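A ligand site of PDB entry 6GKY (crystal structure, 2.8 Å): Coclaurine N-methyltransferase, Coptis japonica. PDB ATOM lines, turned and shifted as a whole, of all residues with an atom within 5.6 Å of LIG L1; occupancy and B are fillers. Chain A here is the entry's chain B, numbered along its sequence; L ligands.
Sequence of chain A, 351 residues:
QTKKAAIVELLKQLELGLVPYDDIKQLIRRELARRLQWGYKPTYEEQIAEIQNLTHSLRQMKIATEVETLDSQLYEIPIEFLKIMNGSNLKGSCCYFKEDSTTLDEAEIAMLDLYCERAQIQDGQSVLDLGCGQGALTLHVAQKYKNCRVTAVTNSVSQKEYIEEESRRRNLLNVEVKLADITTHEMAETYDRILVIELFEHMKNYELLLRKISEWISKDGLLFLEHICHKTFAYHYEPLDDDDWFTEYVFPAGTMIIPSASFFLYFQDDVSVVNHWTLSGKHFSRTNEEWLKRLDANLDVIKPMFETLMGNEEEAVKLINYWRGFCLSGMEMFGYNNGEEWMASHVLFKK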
ATOM      1  N   ALA A  64       6.789  15.653  -1.253  1.00  0.00           N
ATOM      2  CA  ALA A  64       7.298  15.186  -2.530  1.00  0.00           C
ATOM      3  C   ALA A  64       8.716  15.673  -2.766  1.00  0.00           C
ATOM      4  O   ALA A  64       8.982  16.872  -2.680  1.00  0.00           O
ATOM      5  CB  ALA A  64       6.391  15.640  -3.660  1.00  0.00           C
ATOM      6  N   VAL A  67      10.352  17.117  -7.311  1.00  0.00           N
ATOM      7  CA  VAL A  67       9.379  18.138  -7.657  1.00  0.00           C
ATOM      8  C   VAL A  67       9.708  19.054  -8.836  1.00  0.00           C
ATOM      9  O   VAL A  67       8.785  19.600  -9.460  1.00  0.00           O
ATOM     10  CB  VAL A  67       9.082  19.035  -6.455  1.00  0.00           C
ATOM     11  CG1 VAL A  67      10.269  19.942  -6.196  1.00  0.00           C
ATOM     12  CG2 VAL A  67       7.818  19.850  -6.705  1.00  0.00           C
ATOM     13  N   ASP A  71       8.333  17.404 -14.348  1.00  0.00           N
ATOM     14  CA  ASP A  71       7.618  17.331 -15.595  1.00  0.00           C
ATOM     15  C   ASP A  71       8.393  18.128 -16.648  1.00  0.00           C
ATOM     16  O   ASP A  71       7.821  18.750 -17.548  1.00  0.00           O
ATOM     17  CB  ASP A  71       6.172  17.861 -15.474  1.00  0.00           C
ATOM     18  CG  ASP A  71       6.060  19.410 -15.562  1.00  0.00           C
ATOM     19  OD1 ASP A  71       5.336  19.887 -16.492  1.00  0.00           O
ATOM     20  OD2 ASP A  71       6.714  20.119 -14.733  1.00  0.00           O
ATOM     21  N   TYR A  75       5.361  15.533 -18.466  1.00  0.00           N
ATOM     22  CA  TYR A  75       4.324  16.580 -18.389  1.00  0.00           C
ATOM     23  C   TYR A  75       4.535  17.969 -19.034  1.00  0.00           C
ATOM     24  O   TYR A  75       3.571  18.726 -19.165  1.00  0.00           O
ATOM     25  CB  TYR A  75       3.975  16.788 -16.916  1.00  0.00           C
ATOM     26  CG  TYR A  75       3.566  15.535 -16.189  1.00  0.00           C
ATOM     27  CD1 TYR A  75       2.669  14.657 -16.764  1.00  0.00           C
ATOM     28  CD2 TYR A  75       4.088  15.225 -14.936  1.00  0.00           C
ATOM     29  CE1 TYR A  75       2.296  13.504 -16.107  1.00  0.00           C
ATOM     30  CE2 TYR A  75       3.715  14.072 -14.278  1.00  0.00           C
ATOM     31  CZ  TYR A  75       2.809  13.211 -14.869  1.00  0.00           C
ATOM     32  OH  TYR A  75       2.420  12.056 -14.238  1.00  0.00           O
ATOM     33  N   LEU A  90      -7.915  14.951 -24.415  1.00  0.00           N
ATOM     34  CA  LEU A  90      -6.521  14.947 -23.989  1.00  0.00           C
ATOM     35  C   LEU A  90      -6.366  14.432 -22.562  1.00  0.00           C
ATOM     36  O   LEU A  90      -5.715  15.054 -21.728  1.00  0.00           O
ATOM     37  CB  LEU A  90      -5.923  16.360 -24.098  1.00  0.00           C
ATOM     38  CG  LEU A  90      -6.023  17.027 -25.464  1.00  0.00           C
ATOM     39  CD1 LEU A  90      -5.278  18.349 -25.468  1.00  0.00           C
ATOM     40  CD2 LEU A  90      -5.493  16.115 -26.558  1.00  0.00           C
ATOM     41  N   LYS A  91      -6.977  13.282 -22.290  1.00  0.00           N
ATOM     42  CA  LYS A  91      -6.927  12.668 -20.963  1.00  0.00           C
ATOM     43  C   LYS A  91      -5.671  11.826 -20.820  1.00  0.00           C
ATOM     44  O   LYS A  91      -5.563  10.741 -21.405  1.00  0.00           O
ATOM     45  CB  LYS A  91      -8.178  11.831 -20.707  1.00  0.00           C
ATOM     46  CG  LYS A  91      -8.411  11.483 -19.242  1.00  0.00           C
ATOM     47  CD  LYS A  91      -9.714  10.737 -19.052  1.00  0.00           C
ATOM     48  CE  LYS A  91     -10.089  10.613 -17.580  1.00  0.00           C
ATOM     49  NZ  LYS A  91      -9.051   9.926 -16.785  1.00  0.00           N
ATOM     50  N   GLY A  92      -4.713  12.321 -20.039  1.00  0.00           N
ATOM     51  CA  GLY A  92      -3.460  11.621 -19.829  1.00  0.00           C
ATOM     52  C   GLY A  92      -3.541  10.574 -18.734  1.00  0.00           C
ATOM     53  O   GLY A  92      -2.534  10.224 -18.128  1.00  0.00           O
ATOM     54  N   SER A  93      -4.750  10.072 -18.491  1.00  0.00           N
ATOM     55  CA  SER A  93      -4.974   9.064 -17.466  1.00  0.00           C
ATOM     56  C   SER A  93      -5.875   7.956 -17.980  1.00  0.00           C
ATOM     57  O   SER A  93      -6.239   7.928 -19.150  1.00  0.00           O
ATOM     58  CB  SER A  93      -5.570   9.707 -16.214  1.00  0.00           C
ATOM     59  OG  SER A  93      -6.767  10.405 -16.512  1.00  0.00           O
ATOM     60  N   ASP A 129      -9.665  20.820  -9.179  1.00  0.00           N
ATOM     61  CA  ASP A 129      -8.998  19.737  -9.887  1.00  0.00           C
ATOM     62  C   ASP A 129      -7.477  19.812  -9.735  1.00  0.00           C
ATOM     63  O   ASP A 129      -6.796  20.468 -10.533  1.00  0.00           O
ATOM     64  CB  ASP A 129      -9.378  19.774 -11.375  1.00  0.00           C
ATOM     65  CG  ASP A 129      -8.808  18.603 -12.159  1.00  0.00           C
ATOM     66  OD1 ASP A 129      -8.449  17.583 -11.535  1.00  0.00           O
ATOM     67  OD2 ASP A 129      -8.720  18.699 -13.396  1.00  0.00           O
ATOM     68  N   LEU A 130      -6.959  19.148  -8.708  1.00  0.00           N
ATOM     69  CA  LEU A 130      -5.526  19.102  -8.460  1.00  0.00           C
ATOM     70  C   LEU A 130      -4.837  18.199  -9.472  1.00  0.00           C
ATOM     71  O   LEU A 130      -5.234  17.050  -9.662  1.00  0.00           O
ATOM     72  CB  LEU A 130      -5.241  18.636  -7.036  1.00  0.00           C
ATOM     73  CG  LEU A 130      -5.770  19.518  -5.910  1.00  0.00           C
ATOM     74  CD1 LEU A 130      -5.487  18.896  -4.553  1.00  0.00           C
ATOM     75  CD2 LEU A 130      -5.164  20.914  -6.004  1.00  0.00           C
ATOM     76  N   GLY A 131      -3.792  18.717 -10.120  1.00  0.00           N
ATOM     77  CA  GLY A 131      -3.127  17.992 -11.185  1.00  0.00           C
ATOM     78  C   GLY A 131      -4.091  17.789 -12.337  1.00  0.00           C
ATOM     79  O   GLY A 131      -4.437  16.669 -12.696  1.00  0.00           O
ATOM     80  N   CYS A 132      -4.522  18.899 -12.929  1.00  0.00           N
ATOM     81  CA  CYS A 132      -5.575  18.887 -13.942  1.00  0.00           C
ATOM     82  C   CYS A 132      -5.099  18.379 -15.295  1.00  0.00           C
ATOM     83  O   CYS A 132      -5.919  18.026 -16.156  1.00  0.00           O
ATOM     84  CB  CYS A 132      -6.159  20.296 -14.096  1.00  0.00           C
ATOM     85  SG  CYS A 132      -4.937  21.572 -14.489  1.00  0.00           S
ATOM     86  N   GLY A 133      -3.786  18.328 -15.495  1.00  0.00           N
ATOM     87  CA  GLY A 133      -3.239  17.923 -16.774  1.00  0.00           C
ATOM     88  C   GLY A 133      -3.613  18.913 -17.862  1.00  0.00           C
ATOM     89  O   GLY A 133      -3.449  20.122 -17.686  1.00  0.00           O
ATOM     90  N   GLN A 134      -4.121  18.411 -18.986  1.00  0.00           N
ATOM     91  CA  GLN A 134      -4.536  19.273 -20.085  1.00  0.00           C
ATOM     92  C   GLN A 134      -5.986  19.722 -19.890  1.00  0.00           C
ATOM     93  O   GLN A 134      -6.605  20.277 -20.807  1.00  0.00           O
ATOM     94  CB  GLN A 134      -4.379  18.561 -21.426  1.00  0.00           C
ATOM     95  CG  GLN A 134      -2.934  18.180 -21.746  1.00  0.00           C
ATOM     96  CD  GLN A 134      -2.026  19.392 -21.878  1.00  0.00           C
ATOM     97  OE1 GLN A 134      -2.491  20.504 -22.093  1.00  0.00           O
ATOM     98  NE2 GLN A 134      -0.728  19.167 -21.737  1.00  0.00           N
ATOM     99  N   ALA A 136      -8.759  17.806 -19.056  1.00  0.00           N
ATOM    100  CA  ALA A 136      -9.780  16.907 -19.587  1.00  0.00           C
ATOM    101  C   ALA A 136     -10.997  16.866 -18.677  1.00  0.00           C
ATOM    102  O   ALA A 136     -12.144  16.799 -19.144  1.00  0.00           O
ATOM    103  CB  ALA A 136      -9.213  15.513 -19.787  1.00  0.00           C
ATOM    104  N   VAL A 153      -5.559  23.305 -10.997  1.00  0.00           N
ATOM    105  CA  VAL A 153      -4.248  23.623 -10.427  1.00  0.00           C
ATOM    106  C   VAL A 153      -3.148  22.826 -11.117  1.00  0.00           C
ATOM    107  O   VAL A 153      -3.264  21.617 -11.305  1.00  0.00           O
ATOM    108  CB  VAL A 153      -4.211  23.338  -8.905  1.00  0.00           C
ATOM    109  CG1 VAL A 153      -2.806  23.560  -8.361  1.00  0.00           C
ATOM    110  CG2 VAL A 153      -5.217  24.209  -8.181  1.00  0.00           C
ATOM    111  N   THR A 154      -2.077  23.520 -11.486  1.00  0.00           N
ATOM    112  CA  THR A 154      -0.956  22.879 -12.164  1.00  0.00           C
ATOM    113  C   THR A 154       0.357  23.598 -11.875  1.00  0.00           C
ATOM    114  O   THR A 154       0.370  24.794 -11.603  1.00  0.00           O
ATOM    115  CB  THR A 154      -1.167  22.826 -13.684  1.00  0.00           C
ATOM    116  OG1 THR A 154      -2.518  22.430 -13.973  1.00  0.00           O
ATOM    117  CG2 THR A 154      -0.209  21.829 -14.321  1.00  0.00           C
ATOM    118  N   ASN A 155       1.462  22.856 -11.939  1.00  0.00           N
ATOM    119  CA  ASN A 155       2.781  23.456 -11.861  1.00  0.00           C
ATOM    120  C   ASN A 155       3.403  23.524 -13.250  1.00  0.00           C
ATOM    121  O   ASN A 155       4.536  23.975 -13.429  1.00  0.00           O
ATOM    122  CB  ASN A 155       3.684  22.670 -10.912  1.00  0.00           C
ATOM    123  CG  ASN A 155       3.975  21.260 -11.404  1.00  0.00           C
ATOM    124  OD1 ASN A 155       3.175  20.670 -12.132  1.00  0.00           O
ATOM    125  ND2 ASN A 155       5.122  20.718 -11.010  1.00  0.00           N
ATOM    126  N   SER A 156       2.634  23.066 -14.234  1.00  0.00           N
ATOM    127  CA  SER A 156       3.063  23.085 -15.633  1.00  0.00           C
ATOM    128  C   SER A 156       2.589  24.364 -16.318  1.00  0.00           C
ATOM    129  O   SER A 156       1.414  24.720 -16.232  1.00  0.00           O
ATOM    130  CB  SER A 156       2.531  21.862 -16.371  1.00  0.00           C
ATOM    131  OG  SER A 156       2.913  21.895 -17.740  1.00  0.00           O
ATOM    132  N   GLN A 159       0.446  23.541 -19.501  1.00  0.00           N
ATOM    133  CA  GLN A 159      -0.814  22.921 -19.126  1.00  0.00           C
ATOM    134  C   GLN A 159      -1.792  23.999 -18.665  1.00  0.00           C
ATOM    135  O   GLN A 159      -2.994  23.905 -18.905  1.00  0.00           O
ATOM    136  CB  GLN A 159      -0.626  21.878 -18.018  1.00  0.00           C
ATOM    137  CG  GLN A 159       0.026  20.584 -18.490  1.00  0.00           C
ATOM    138  CD  GLN A 159      -0.078  19.471 -17.461  1.00  0.00           C
ATOM    139  OE1 GLN A 159      -0.717  19.632 -16.423  1.00  0.00           O
ATOM    140  NE2 GLN A 159       0.557  18.345 -17.753  1.00  0.00           N
ATOM    141  N   ALA A 180       0.949  26.754  -9.677  1.00  0.00           N
ATOM    142  CA  ALA A 180       1.533  26.505  -8.367  1.00  0.00           C
ATOM    143  C   ALA A 180       1.994  25.069  -8.155  1.00  0.00           C
ATOM    144  O   ALA A 180       1.509  24.134  -8.800  1.00  0.00           O
ATOM    145  CB  ALA A 180       0.540  26.896  -7.276  1.00  0.00           C
ATOM    146  N   ASP A 181       2.933  24.909  -7.228  1.00  0.00           N
ATOM    147  CA  ASP A 181       3.410  23.601  -6.808  1.00  0.00           C
ATOM    148  C   ASP A 181       2.603  23.146  -5.595  1.00  0.00           C
ATOM    149  O   ASP A 181       2.690  23.745  -4.518  1.00  0.00           O
ATOM    150  CB  ASP A 181       4.908  23.660  -6.493  1.00  0.00           C
ATOM    151  CG  ASP A 181       5.479  22.321  -6.067  1.00  0.00           C
ATOM    152  OD1 ASP A 181       4.759  21.303  -6.096  1.00  0.00           O
ATOM    153  OD2 ASP A 181       6.666  22.308  -5.670  1.00  0.00           O
ATOM    154  N   ILE A 182       1.827  22.079  -5.763  1.00  0.00           N
ATOM    155  CA  ILE A 182       0.942  21.591  -4.707  1.00  0.00           C
ATOM    156  C   ILE A 182       1.729  21.145  -3.475  1.00  0.00           C
ATOM    157  O   ILE A 182       1.191  21.065  -2.374  1.00  0.00           O
ATOM    158  CB  ILE A 182       0.066  20.423  -5.205  1.00  0.00           C
ATOM    159  CG1 ILE A 182      -0.713  20.845  -6.452  1.00  0.00           C
ATOM    160  CG2 ILE A 182      -0.899  19.960  -4.116  1.00  0.00           C
ATOM    161  CD1 ILE A 182      -1.669  19.777  -6.963  1.00  0.00           C
ATOM    162  N   THR A 183       3.015  20.851  -3.664  1.00  0.00           N
ATOM    163  CA  THR A 183       3.878  20.425  -2.570  1.00  0.00           C
ATOM    164  C   THR A 183       4.056  21.537  -1.537  1.00  0.00           C
ATOM    165  O   THR A 183       4.078  21.281  -0.329  1.00  0.00           O
ATOM    166  CB  THR A 183       5.262  19.998  -3.079  1.00  0.00           C
ATOM    167  OG1 THR A 183       5.123  18.844  -3.928  1.00  0.00           O
ATOM    168  CG2 THR A 183       6.179  19.659  -1.913  1.00  0.00           C
ATOM    169  N   ILE A 197      -6.799  13.236  -9.800  1.00  0.00           N
ATOM    170  CA  ILE A 197      -6.736  12.115 -10.731  1.00  0.00           C
ATOM    171  C   ILE A 197      -5.291  11.704 -11.019  1.00  0.00           C
ATOM    172  O   ILE A 197      -4.608  12.330 -11.827  1.00  0.00           O
ATOM    173  CB  ILE A 197      -7.427  12.457 -12.059  1.00  0.00           C
ATOM    174  CG1 ILE A 197      -8.844  12.970 -11.807  1.00  0.00           C
ATOM    175  CG2 ILE A 197      -7.448  11.236 -12.973  1.00  0.00           C
ATOM    176  CD1 ILE A 197      -9.709  12.017 -11.001  1.00  0.00           C
ATOM    177  N   GLU A 198      -4.853  10.629 -10.357  1.00  0.00           N
ATOM    178  CA  GLU A 198      -3.524  10.077 -10.572  1.00  0.00           C
ATOM    179  C   GLU A 198      -2.425  11.108 -10.312  1.00  0.00           C
ATOM    180  O   GLU A 198      -1.588  11.374 -11.173  1.00  0.00           O
ATOM    181  CB  GLU A 198      -3.400   9.524 -12.002  1.00  0.00           C
ATOM    182  CG  GLU A 198      -4.381   8.419 -12.314  1.00  0.00           C
ATOM    183  CD  GLU A 198      -4.173   7.803 -13.685  1.00  0.00           C
ATOM    184  OE1 GLU A 198      -3.187   8.184 -14.361  1.00  0.00           O
ATOM    185  OE2 GLU A 198      -4.972   6.944 -14.086  1.00  0.00           O
ATOM    186  N   LEU A 199      -2.438  11.671  -9.107  1.00  0.00           N
ATOM    187  CA  LEU A 199      -1.447  12.662  -8.713  1.00  0.00           C
ATOM    188  C   LEU A 199      -0.604  12.161  -7.542  1.00  0.00           C
ATOM    189  O   LEU A 199       0.556  12.528  -7.407  1.00  0.00           O
ATOM    190  CB  LEU A 199      -2.130  13.988  -8.339  1.00  0.00           C
ATOM    191  CG  LEU A 199      -1.244  15.063  -7.714  1.00  0.00           C
ATOM    192  CD1 LEU A 199      -0.265  15.625  -8.736  1.00  0.00           C
ATOM    193  CD2 LEU A 199      -2.090  16.173  -7.101  1.00  0.00           C
ATOM    194  N   HIS A 202       2.936  10.428  -7.591  1.00  0.00           N
ATOM    195  CA  HIS A 202       4.147  11.247  -7.671  1.00  0.00           C
ATOM    196  C   HIS A 202       4.558  11.802  -6.317  1.00  0.00           C
ATOM    197  O   HIS A 202       5.649  12.346  -6.156  1.00  0.00           O
ATOM    198  CB  HIS A 202       3.929  12.403  -8.657  1.00  0.00           C
ATOM    199  CG  HIS A 202       3.675  11.955 -10.060  1.00  0.00           C
ATOM    200  ND1 HIS A 202       4.543  11.135 -10.747  1.00  0.00           N
ATOM    201  CD2 HIS A 202       2.657  12.227 -10.917  1.00  0.00           C
ATOM    202  CE1 HIS A 202       4.064  10.912 -11.966  1.00  0.00           C
ATOM    203  NE2 HIS A 202       2.922  11.563 -12.082  1.00  0.00           N
ATOM    204  N   MET A 203       3.678  11.660  -5.319  1.00  0.00           N
ATOM    205  CA  MET A 203       3.939  12.218  -3.999  1.00  0.00           C
ATOM    206  C   MET A 203       4.573  11.184  -3.076  1.00  0.00           C
ATOM    207  O   MET A 203       4.688  10.014  -3.422  1.00  0.00           O
ATOM    208  CB  MET A 203       2.655  12.770  -3.394  1.00  0.00           C
ATOM    209  CG  MET A 203       1.948  13.767  -4.277  1.00  0.00           C
ATOM    210  SD  MET A 203       2.986  15.184  -4.691  1.00  0.00           S
ATOM    211  CE  MET A 203       2.514  15.436  -6.403  1.00  0.00           C
HETATM  212  N1  LIG L   1      -5.192  14.777 -14.067  1.00  0.00           N
HETATM  213  C1  LIG L   1      -4.732  14.867 -15.446  1.00  0.00           C
HETATM  214  C2  LIG L   1      -3.236  14.603 -15.537  1.00  0.00           C
HETATM  215  C3  LIG L   1      -2.743  13.465 -14.644  1.00  0.00           C
HETATM  216  S1  LIG L   1      -0.968  13.187 -14.814  1.00  0.00           S
HETATM  217  C4  LIG L   1      -5.495  13.896 -16.347  1.00  0.00           C
HETATM  218  O1  LIG L   1      -6.151  12.974 -15.869  1.00  0.00           O
HETATM  219  O2  LIG L   1      -5.476  14.020 -17.573  1.00  0.00           O
HETATM  220  C5  LIG L   1      -0.698  14.000 -13.219  1.00  0.00           C
HETATM  221  C6  LIG L   1      -0.718  15.527 -13.337  1.00  0.00           C
HETATM  222  O3  LIG L   1      -0.349  16.110 -12.102  1.00  0.00           O
HETATM  223  C7  LIG L   1       0.254  16.018 -14.385  1.00  0.00           C
HETATM  224  O4  LIG L   1      -0.443  16.642 -15.432  1.00  0.00           O
HETATM  225  C8  LIG L   1       1.150  17.022 -13.694  1.00  0.00           C
HETATM  226  O5  LIG L   1       1.151  18.248 -14.393  1.00  0.00           O
HETATM  227  C9  LIG L   1       0.532  17.205 -12.321  1.00  0.00           C
HETATM  228  N2  LIG L   1       1.576  17.257 -11.278  1.00  0.00           N
HETATM  229  C10 LIG L   1       2.540  16.306 -11.039  1.00  0.00           C
HETATM  230  N3  LIG L   1       3.302  16.721 -10.006  1.00  0.00           N
HETATM  231  C11 LIG L   1       2.845  17.917  -9.578  1.00  0.00           C
HETATM  232  C12 LIG L   1       3.266  18.766  -8.568  1.00  0.00           C
HETATM  233  N4  LIG L   1       4.307  18.449  -7.809  1.00  0.00           N
HETATM  234  N5  LIG L   1       2.588  19.958  -8.355  1.00  0.00           N
HETATM  235  C13 LIG L   1       1.515  20.285  -9.152  1.00  0.00           C
HETATM  236  N6  LIG L   1       1.108  19.439 -10.159  1.00  0.00           N
HETATM  237  C14 LIG L   1       1.760  18.263 -10.373  1.00  0.00           C
HETATM  238  C1  LG2 L   2       2.372   2.599 -13.574  1.00  0.00           C
HETATM  239  O1  LG2 L   2       2.403   3.077 -14.928  1.00  0.00           O
HETATM  240  C2  LG2 L   2       1.744   4.250 -15.136  1.00  0.00           C
HETATM  241  C3  LG2 L   2       1.398   5.141 -14.123  1.00  0.00           C
HETATM  242  C4  LG2 L   2       0.723   6.319 -14.437  1.00  0.00           C
HETATM  243  C5  LG2 L   2       0.385   7.185 -13.397  1.00  0.00           C
HETATM  244  C6  LG2 L   2       0.385   8.514 -13.812  1.00  0.00           C
HETATM  245  O2  LG2 L   2       0.662   9.410 -13.015  1.00  0.00           O
HETATM  246  N1  LG2 L   2       0.067   8.842 -15.139  1.00  0.00           N
HETATM  247  C7  LG2 L   2      -0.277   7.776 -16.099  1.00  0.00           C
HETATM  248  C8  LG2 L   2       0.399   6.612 -15.769  1.00  0.00           C
HETATM  249  C9  LG2 L   2       0.751   5.719 -16.774  1.00  0.00           C
HETATM  250  C10 LG2 L   2       1.431   4.554 -16.461  1.00  0.00           C
HETATM  251  O3  LG2 L   2       1.785   3.630 -17.410  1.00  0.00           O
HETATM  252  C11 LG2 L   2       3.167   3.684 -17.773  1.00  0.00           C
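SG of Cys 132 sits at hydrogen-bond distance from OG1 of Thr 154 (2.6 Å). The backbone NH (N) of Cys 132 lies within hydrogen-bond range of the backbone carbonyl oxygen (O) of Val 153. The backbone carbonyl oxygen (O) of Ala 180 sits close to the backbone NH (N) of Asn 155, 3.4 Å away. The side-chain amide oxygen of Gln 159 sits close to the backbone carbonyl oxygen of Gly 133 (3.0 Å). N of Gly 131 sits at hydrogen-bond distance from O of Val 153 (3.2 Å). The backbone NH (N) of Ala 180 is in hydrogen-bond range of the backbone carbonyl oxygen (O) of Thr 154 (2.8 Å). The side-chain hydroxyl (OG) of Ser 156 sits close to the backbone NH (N) of Gln 159. The side-chain amide nitrogen (NE2) of Gln 159 lies within hydrogen-bond range of the backbone carbonyl oxygen (O) of Tyr 75 (3.4 Å).
Merely in contact with LIG L1: Gly 133, Leu 199, Glu 198, Cys 132, Met 203, Thr 154, Ala 180, Lys 91, Val 67 and Thr 183. Hydrophobic or aromatic side chains within 4 Å of LIG L1: Val 67, Tyr 75, Ile 182, Ile 197, Leu 199 and Met 203. The nearest printed residue that does not touch LIG L1 is His 202 (4.1 Å).
The backbone carbonyl oxygen (O) of Gly 131 sits at hydrogen-bond distance from a nitrogen (N1) of LIG L1 (2.5 Å). OE1 of Glu 198 sits at hydrogen-bond distance from N1 of LG2 L2 (3.4 Å). OH of Tyr 75 sits close to S1 of LIG L1, at 3.6 Å. N of Ile 182 is in hydrogen-bond range of N5 of LIG L1 (3.4 Å). An oxygen (O2) of LIG L1 is in hydrogen-bond range of the backbone NH (N) of Gly 92. A nitrogen (N6) of LIG L1 sits close to the side-chain amide oxygen (OD1) of Asn 155 (3.1 Å). OG of Ser 93 lies within hydrogen-bond range of O1 of LIG L1 (2.7 Å). The side-chain hydroxyl (OH) of Tyr 75 is in hydrogen-bond range of an oxygen (O2) of LG2 L2 (3.4 Å). NE2 of His 202 is in hydrogen-bond range of O2 of LG2 L2 (3.3 Å). The backbone carbonyl oxygen (O) of Ile 197 is in hydrogen-bond range of a nitrogen (N1) of LIG L1 (3.4 Å). The side-chain amide nitrogen of Gln 159 lies within hydrogen-bond range of an oxygen (O4) of LIG L1 (3.0 Å). The side-chain carboxylate of Asp 181 sits at hydrogen-bond distance from a nitrogen (N4) of LIG L1 (3.4 Å).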
